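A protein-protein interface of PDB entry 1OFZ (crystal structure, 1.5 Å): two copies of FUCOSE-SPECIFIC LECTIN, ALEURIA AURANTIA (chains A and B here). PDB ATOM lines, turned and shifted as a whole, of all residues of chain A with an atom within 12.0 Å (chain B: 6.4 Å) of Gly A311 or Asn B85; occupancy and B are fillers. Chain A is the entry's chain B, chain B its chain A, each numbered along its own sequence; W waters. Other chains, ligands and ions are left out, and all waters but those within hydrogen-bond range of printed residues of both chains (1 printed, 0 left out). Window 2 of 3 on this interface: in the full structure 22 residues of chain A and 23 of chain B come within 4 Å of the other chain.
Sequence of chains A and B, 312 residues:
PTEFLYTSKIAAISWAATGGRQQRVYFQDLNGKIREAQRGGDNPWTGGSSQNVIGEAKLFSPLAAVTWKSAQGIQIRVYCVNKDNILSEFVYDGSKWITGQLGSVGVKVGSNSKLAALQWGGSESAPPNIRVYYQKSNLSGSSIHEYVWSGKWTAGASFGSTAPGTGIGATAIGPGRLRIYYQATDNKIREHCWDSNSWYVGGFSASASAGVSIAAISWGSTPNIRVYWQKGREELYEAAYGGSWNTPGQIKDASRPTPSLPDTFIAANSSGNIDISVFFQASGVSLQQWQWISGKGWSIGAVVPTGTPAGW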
ATOM      1  N   PRO A   1       1.731  18.781  21.332  1.00  0.00           N
ATOM      2  CA  PRO A   1       0.559  18.058  21.935  1.00  0.00           C
ATOM      3  C   PRO A   1      -0.792  18.602  21.477  1.00  0.00           C
ATOM      4  O   PRO A   1      -0.877  19.713  20.911  1.00  0.00           O
ATOM      5  CB  PRO A   1       0.748  18.276  23.432  1.00  0.00           C
ATOM      6  CG  PRO A   1       1.578  19.472  23.551  1.00  0.00           C
ATOM      7  CD  PRO A   1       2.459  19.554  22.346  1.00  0.00           C
ATOM      8  N   THR A   2      -1.848  17.828  21.732  1.00  0.00           N
ATOM      9  CA  THR A   2      -3.222  18.189  21.418  1.00  0.00           C
ATOM     10  C   THR A   2      -4.141  17.950  22.601  1.00  0.00           C
ATOM     11  O   THR A   2      -3.705  17.483  23.632  1.00  0.00           O
ATOM     12  CB  THR A   2      -3.779  17.391  20.230  1.00  0.00           C
ATOM     13  OG1 THR A   2      -4.080  16.067  20.656  1.00  0.00           O
ATOM     14  CG2 THR A   2      -2.780  17.227  19.096  1.00  0.00           C
ATOM     15  N   GLU A   3      -5.424  18.231  22.399  1.00  0.00           N
ATOM     16  CA  GLU A   3      -6.446  18.017  23.396  1.00  0.00           C
ATOM     17  C   GLU A   3      -7.206  16.725  23.158  1.00  0.00           C
ATOM     18  O   GLU A   3      -8.201  16.471  23.781  1.00  0.00           O
ATOM     19  CB  GLU A   3      -7.384  19.228  23.417  1.00  0.00           C
ATOM     20  CG  GLU A   3      -6.621  20.468  23.796  1.00  0.00           C
ATOM     21  CD  GLU A   3      -7.438  21.742  23.751  1.00  0.00           C
ATOM     22  OE1 GLU A   3      -8.338  21.895  22.884  1.00  0.00           O
ATOM     23  OE2 GLU A   3      -7.171  22.605  24.613  1.00  0.00           O
ATOM     24  N   LEU A  30      -9.677  15.942  26.598  1.00  0.00           N
ATOM     25  CA  LEU A  30      -9.109  15.674  27.916  1.00  0.00           C
ATOM     26  C   LEU A  30     -10.104  15.956  29.037  1.00  0.00           C
ATOM     27  O   LEU A  30     -10.013  15.385  30.134  1.00  0.00           O
ATOM     28  CB  LEU A  30      -7.854  16.508  28.117  1.00  0.00           C
ATOM     29  CG  LEU A  30      -6.731  16.285  27.111  1.00  0.00           C
ATOM     30  CD1 LEU A  30      -5.652  17.309  27.278  1.00  0.00           C
ATOM     31  CD2 LEU A  30      -6.173  14.896  27.241  1.00  0.00           C
ATOM     32  N   GLY A 307      -7.419  20.335  18.592  1.00  0.00           N
ATOM     33  CA  GLY A 307      -7.104  21.342  19.595  1.00  0.00           C
ATOM     34  C   GLY A 307      -5.634  21.400  19.946  1.00  0.00           C
ATOM     35  O   GLY A 307      -4.873  20.427  19.787  1.00  0.00           O
ATOM     36  N   THR A 308      -5.215  22.558  20.439  1.00  0.00           N
ATOM     37  CA  THR A 308      -3.873  22.763  20.948  1.00  0.00           C
ATOM     38  C   THR A 308      -3.995  23.367  22.340  1.00  0.00           C
ATOM     39  O   THR A 308      -4.612  24.399  22.510  1.00  0.00           O
ATOM     40  CB  THR A 308      -3.078  23.714  20.076  1.00  0.00           C
ATOM     41  OG1 THR A 308      -2.951  23.185  18.740  1.00  0.00           O
ATOM     42  CG2 THR A 308      -1.641  23.858  20.596  1.00  0.00           C
ATOM     43  N   PRO A 309      -3.401  22.726  23.344  1.00  0.00           N
ATOM     44  CA  PRO A 309      -3.458  23.254  24.712  1.00  0.00           C
ATOM     45  C   PRO A 309      -2.710  24.585  24.817  1.00  0.00           C
ATOM     46  O   PRO A 309      -1.771  24.883  24.059  1.00  0.00           O
ATOM     47  CB  PRO A 309      -2.769  22.185  25.552  1.00  0.00           C
ATOM     48  CG  PRO A 309      -2.025  21.353  24.614  1.00  0.00           C
ATOM     49  CD  PRO A 309      -2.632  21.471  23.254  1.00  0.00           C
ATOM     50  N   ALA A 310      -3.138  25.371  25.784  1.00  0.00           N
ATOM     51  CA  ALA A 310      -2.469  26.628  26.092  1.00  0.00           C
ATOM     52  C   ALA A 310      -1.005  26.399  26.442  1.00  0.00           C
ATOM     53  O   ALA A 310      -0.659  25.422  27.130  1.00  0.00           O
ATOM     54  CB  ALA A 310      -3.161  27.312  27.220  1.00  0.00           C
ATOM     55  N   GLY A 311      -0.149  27.286  25.924  1.00  0.00           N
ATOM     56  CA  GLY A 311       1.283  27.233  26.140  1.00  0.00           C
ATOM     57  C   GLY A 311       2.046  26.456  25.093  1.00  0.00           C
ATOM     58  O   GLY A 311       3.245  26.211  25.251  1.00  0.00           O
ATOM     59  N   TRP A 312       1.359  26.047  24.020  1.00  0.00           N
ATOM     60  CA  TRP A 312       1.955  25.293  22.942  1.00  0.00           C
ATOM     61  C   TRP A 312       1.617  25.903  21.580  1.00  0.00           C
ATOM     62  O   TRP A 312       2.293  25.521  20.611  1.00  0.00           O
ATOM     63  CB  TRP A 312       1.430  23.869  22.979  1.00  0.00           C
ATOM     64  CG  TRP A 312       1.933  23.106  24.169  1.00  0.00           C
ATOM     65  CD1 TRP A 312       1.307  22.941  25.363  1.00  0.00           C
ATOM     66  CD2 TRP A 312       3.184  22.389  24.272  1.00  0.00           C
ATOM     67  NE1 TRP A 312       2.104  22.194  26.203  1.00  0.00           N
ATOM     68  CE2 TRP A 312       3.254  21.846  25.547  1.00  0.00           C
ATOM     69  CE3 TRP A 312       4.278  22.201  23.415  1.00  0.00           C
ATOM     70  CZ2 TRP A 312       4.315  21.053  25.968  1.00  0.00           C
ATOM     71  CZ3 TRP A 312       5.316  21.354  23.829  1.00  0.00           C
ATOM     72  CH2 TRP A 312       5.351  20.854  25.091  1.00  0.00           C
ATOM     73  OXT TRP A 312       0.691  26.715  21.486  1.00  0.00           O
ATOM     74  N   LYS B  58       0.688  24.124  32.836  1.00  0.00           N
ATOM     75  CA  LYS B  58       0.160  23.922  31.511  1.00  0.00           C
ATOM     76  C   LYS B  58       0.078  22.424  31.247  1.00  0.00           C
ATOM     77  O   LYS B  58       0.884  21.650  31.760  1.00  0.00           O
ATOM     78  CB  LYS B  58       1.030  24.591  30.433  1.00  0.00           C
ATOM     79  CG  LYS B  58       2.354  23.928  30.059  1.00  0.00           C
ATOM     80  CD  LYS B  58       2.959  24.650  28.851  1.00  0.00           C
ATOM     81  CE  LYS B  58       4.172  23.923  28.399  1.00  0.00           C
ATOM     82  NZ  LYS B  58       4.668  24.475  27.095  1.00  0.00           N
ATOM     83  N   VAL B  81       5.918  24.600  34.420  1.00  0.00           N
ATOM     84  CA  VAL B  81       5.735  25.758  33.575  1.00  0.00           C
ATOM     85  C   VAL B  81       4.246  26.064  33.456  1.00  0.00           C
ATOM     86  O   VAL B  81       3.447  25.143  33.185  1.00  0.00           O
ATOM     87  CB  VAL B  81       6.404  25.500  32.191  1.00  0.00           C
ATOM     88  CG1 VAL B  81       5.944  26.434  31.205  1.00  0.00           C
ATOM     89  CG2 VAL B  81       7.935  25.674  32.304  1.00  0.00           C
ATOM     90  N   ASN B  82       3.861  27.331  33.686  1.00  0.00           N
ATOM     91  CA  ASN B  82       2.472  27.718  33.562  1.00  0.00           C
ATOM     92  C   ASN B  82       2.027  27.834  32.103  1.00  0.00           C
ATOM     93  O   ASN B  82       2.814  27.599  31.193  1.00  0.00           O
ATOM     94  CB  ASN B  82       2.165  28.935  34.416  1.00  0.00           C
ATOM     95  CG  ASN B  82       2.667  30.234  33.856  1.00  0.00           C
ATOM     96  OD1 ASN B  82       3.117  30.315  32.703  1.00  0.00           O
ATOM     97  ND2 ASN B  82       2.616  31.283  34.690  1.00  0.00           N
ATOM     98  N   LYS B  83       0.753  28.171  31.884  1.00  0.00           N
ATOM     99  CA  LYS B  83       0.197  28.269  30.531  1.00  0.00           C
ATOM    100  C   LYS B  83       0.766  29.404  29.669  1.00  0.00           C
ATOM    101  O   LYS B  83       0.528  29.435  28.457  1.00  0.00           O
ATOM    102  CB  LYS B  83      -1.324  28.359  30.581  1.00  0.00           C
ATOM    103  CG  LYS B  83      -1.959  27.093  31.127  1.00  0.00           C
ATOM    104  CD  LYS B  83      -3.479  27.188  31.089  1.00  0.00           C
ATOM    105  CE  LYS B  83      -4.107  25.903  31.549  1.00  0.00           C
ATOM    106  NZ  LYS B  83      -5.600  26.044  31.723  1.00  0.00           N
ATOM    107  N   ASP B  84       1.534  30.277  30.290  1.00  0.00           N
ATOM    108  CA  ASP B  84       2.276  31.309  29.589  1.00  0.00           C
ATOM    109  C   ASP B  84       3.776  31.013  29.516  1.00  0.00           C
ATOM    110  O   ASP B  84       4.586  31.904  29.231  1.00  0.00           O
ATOM    111  CB  ASP B  84       1.987  32.643  30.270  1.00  0.00           C
ATOM    112  CG  ASP B  84       0.542  32.989  30.184  1.00  0.00           C
ATOM    113  OD1 ASP B  84       0.031  33.010  29.025  1.00  0.00           O
ATOM    114  OD2 ASP B  84      -0.205  33.119  31.195  1.00  0.00           O
ATOM    115  N   ASN B  85       4.142  29.746  29.706  1.00  0.00           N
ATOM    116  CA  ASN B  85       5.505  29.306  29.601  1.00  0.00           C
ATOM    117  C   ASN B  85       6.458  30.035  30.561  1.00  0.00           C
ATOM    118  O   ASN B  85       7.609  30.324  30.212  1.00  0.00           O
ATOM    119  CB  ASN B  85       5.991  29.372  28.151  1.00  0.00           C
ATOM    120  CG  ASN B  85       5.369  28.306  27.296  1.00  0.00           C
ATOM    121  OD1 ASN B  85       4.741  28.564  26.245  1.00  0.00           O
ATOM    122  ND2 ASN B  85       5.537  27.078  27.750  1.00  0.00           N
ATOM    123  N   ILE B  86       5.971  30.331  31.767  1.00  0.00           N
ATOM    124  CA  ILE B  86       6.790  30.895  32.814  1.00  0.00           C
ATOM    125  C   ILE B  86       7.147  29.789  33.797  1.00  0.00           C
ATOM    126  O   ILE B  86       6.265  29.052  34.270  1.00  0.00           O
ATOM    127  CB  ILE B  86       6.066  32.047  33.558  1.00  0.00           C
ATOM    128  CG1 ILE B  86       5.709  33.188  32.610  1.00  0.00           C
ATOM    129  CG2 ILE B  86       6.868  32.554  34.735  1.00  0.00           C
ATOM    130  CD1 ILE B  86       6.879  33.846  31.951  1.00  0.00           C
ATOM    131  N   LEU B  87       8.420  29.690  34.127  1.00  0.00           N
ATOM    132  CA  LEU B  87       8.902  28.760  35.119  1.00  0.00           C
ATOM    133  C   LEU B  87       8.223  29.057  36.475  1.00  0.00           C
ATOM    134  O   LEU B  87       8.210  30.184  36.945  1.00  0.00           O
ATOM    135  CB  LEU B  87      10.416  28.911  35.213  1.00  0.00           C
ATOM    136  CG  LEU B  87      11.209  27.977  36.071  1.00  0.00           C
ATOM    137  CD1 LEU B  87      10.940  26.520  35.691  1.00  0.00           C
ATOM    138  CD2 LEU B  87      12.688  28.302  35.919  1.00  0.00           C
ATOM    139  N   VAL B 107      10.566  33.944  34.480  1.00  0.00           N
ATOM    140  CA  VAL B 107      11.524  33.276  33.630  1.00  0.00           C
ATOM    141  C   VAL B 107      10.792  32.556  32.507  1.00  0.00           C
ATOM    142  O   VAL B 107      10.042  31.629  32.731  1.00  0.00           O
ATOM    143  CB  VAL B 107      12.374  32.284  34.409  1.00  0.00           C
ATOM    144  CG1 VAL B 107      13.335  31.559  33.470  1.00  0.00           C
ATOM    145  CG2 VAL B 107      13.103  32.987  35.538  1.00  0.00           C
ATOM    146  N   LYS B 108      11.054  32.963  31.278  1.00  0.00           N
ATOM    147  CA  LYS B 108      10.411  32.396  30.124  1.00  0.00           C
ATOM    148  C   LYS B 108      11.133  31.140  29.683  1.00  0.00           C
ATOM    149  O   LYS B 108      12.366  31.097  29.620  1.00  0.00           O
ATOM    150  CB  LYS B 108      10.393  33.396  28.969  1.00  0.00           C
ATOM    151  CG  LYS B 108       9.557  34.636  29.213  1.00  0.00           C
ATOM    152  CD  LYS B 108       9.397  35.440  27.919  1.00  0.00           C
ATOM    153  CE  LYS B 108       8.671  36.764  28.117  1.00  0.00           C
ATOM    154  NZ  LYS B 108       7.449  36.622  28.934  1.00  0.00           N
ATOM    155  N   VAL B 109      10.342  30.124  29.349  1.00  0.00           N
ATOM    156  CA  VAL B 109      10.836  28.794  29.027  1.00  0.00           C
ATOM    157  C   VAL B 109      10.329  28.407  27.649  1.00  0.00           C
ATOM    158  O   VAL B 109       9.148  28.595  27.359  1.00  0.00           O
ATOM    159  CB  VAL B 109      10.300  27.798  30.080  1.00  0.00           C
ATOM    160  CG1 VAL B 109      10.753  26.342  29.747  1.00  0.00           C
ATOM    161  CG2 VAL B 109      10.707  28.255  31.499  1.00  0.00           C
ATOM    162  N   GLY B 110      11.179  27.824  26.796  1.00  0.00           N
ATOM    163  CA  GLY B 110      10.715  27.325  25.513  1.00  0.00           C
ATOM    164  C   GLY B 110       9.539  26.367  25.708  1.00  0.00           C
ATOM    165  O   GLY B 110       9.526  25.568  26.653  1.00  0.00           O
ATOM    166  N   SER B 111       8.562  26.403  24.805  1.00  0.00           N
ATOM    167  CA  SER B 111       7.351  25.587  24.980  1.00  0.00           C
ATOM    168  C   SER B 111       7.656  24.096  25.134  1.00  0.00           C
ATOM    169  O   SER B 111       6.963  23.410  25.904  1.00  0.00           O
ATOM    170  CB  SER B 111       6.356  25.850  23.854  1.00  0.00           C
ATOM    171  OG  SER B 111       6.831  25.394  22.611  1.00  0.00           O
ATOM    172  N   ASN B 112       8.680  23.591  24.455  1.00  0.00           N
ATOM    173  CA  ASN B 112       9.022  22.180  24.482  1.00  0.00           C
ATOM    174  C   ASN B 112      10.208  21.864  25.398  1.00  0.00           C
ATOM    175  O   ASN B 112      10.762  20.776  25.355  1.00  0.00           O
ATOM    176  CB  ASN B 112       9.296  21.660  23.077  1.00  0.00           C
ATOM    177  CG  ASN B 112       9.282  20.147  23.009  1.00  0.00           C
ATOM    178  OD1 ASN B 112       8.406  19.519  23.642  1.00  0.00           O
ATOM    179  ND2 ASN B 112      10.190  19.538  22.222  1.00  0.00           N
HETATM  180  O   HOH W   1       5.063  24.887  20.819  1.00  0.00           O
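The backbone carbonyl oxygen of Val B81 lies within hydrogen-bond range of the backbone NH of Lys B58, at 3.0 Å.
The side-chain amino group (NZ) of Lys B58 sits close to the side-chain amide nitrogen (ND2) of Asn B85.
The side-chain amino group (NZ) of Lys B58 sits at hydrogen-bond distance from the backbone carbonyl oxygen (O) of Ser B111 (2.8 Å).
N of Asn B85 is in hydrogen-bond range of OD1 of Asn B82.
N of Val B109 sits at hydrogen-bond distance from O of Asn B85 (2.9 Å).
NZ of Lys B58 is in hydrogen-bond range of O of Gly A311 (2.9 Å).
The backbone NH (N) of Gly A311 sits close to the backbone carbonyl oxygen (O) of Lys B83 (3.4 Å).
The side-chain amide oxygen (OD1) of Asn B85 sits close to the backbone carbonyl oxygen (O) of Gly A311 (3.0 Å).
Water W1 lies within hydrogen-bond range of OG of Ser B111 (2.6 Å) and O of Trp A312 (2.8 Å).
No position is printed for both chains.
Of the 9 pairs that touch across the chains among the printed residues, none has its exchanged pair printed and touching as well.
Among the printed residues, merely in contact across the chains: Ala A310 with Lys B58 (3.8 Å), Ala A310 with Lys B83 (3.9 Å), Gly A311 with Ser B111 (3.4 Å), Trp A312 with Lys B58 (3.4 Å), Trp A312 with Ser B111 (3.1 Å) and Trp A312 with Asn B112 (3.6 Å).
Of the 10 printed residues of chain A, 3 touch a printed residue of chain B.
Printed residues of chain A that touch a printed residue of chain B: Ala A310, Gly A311 and Trp A312.
Hydrophobic or aromatic side chains of chain A within 4 Å of the printed part of chain B: Ala A310 and Trp A312.
Among the printed residues, 9 pairs touch across the chains.
Among the printed residues, no Asp or Glu carboxylate lies within 4 Å of a Lys or Arg side-chain nitrogen of the other chain.
Printed residues of chain B within 4 Å of Gly A311: Lys B58 (2.9 Å), Lys B83 (3.3 Å), Asn B85 (3.0 Å) and Ser B111 (3.4 Å).
Of chain A, only Gly A311 comes within 4 Å of Asn B85.
Of chain A, only Ala A310 (3.8 Å), Gly A311 (2.9 Å) and Trp A312 (3.4 Å) come within 4 Å of Lys B58.
No residue of chain A comes within 4 Å of Asn B82.
No residue of chain A comes within 4 Å of Asp B84.
No residue of chain A comes within 4 Å of Ile B86.
Printed residues of chain A within 4 Å of Asn B112: Trp A312 (3.6 Å).
Printed residues of chain B within 4 Å of Ala A310: Lys B58 (3.8 Å) and Lys B83 (3.9 Å).
Of the printed residues of chain A, Lys B83 touches Ala A310 (3.9 Å) and Gly A311 (3.3 Å).
Of the printed residues of chain B, Trp A312 touches Lys B58 (3.4 Å), Ser B111 (3.1 Å) and Asn B112 (3.6 Å).
Leu A30 touches none of the printed residues of chain B.
Val B109 touches none of the printed residues of chain A.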
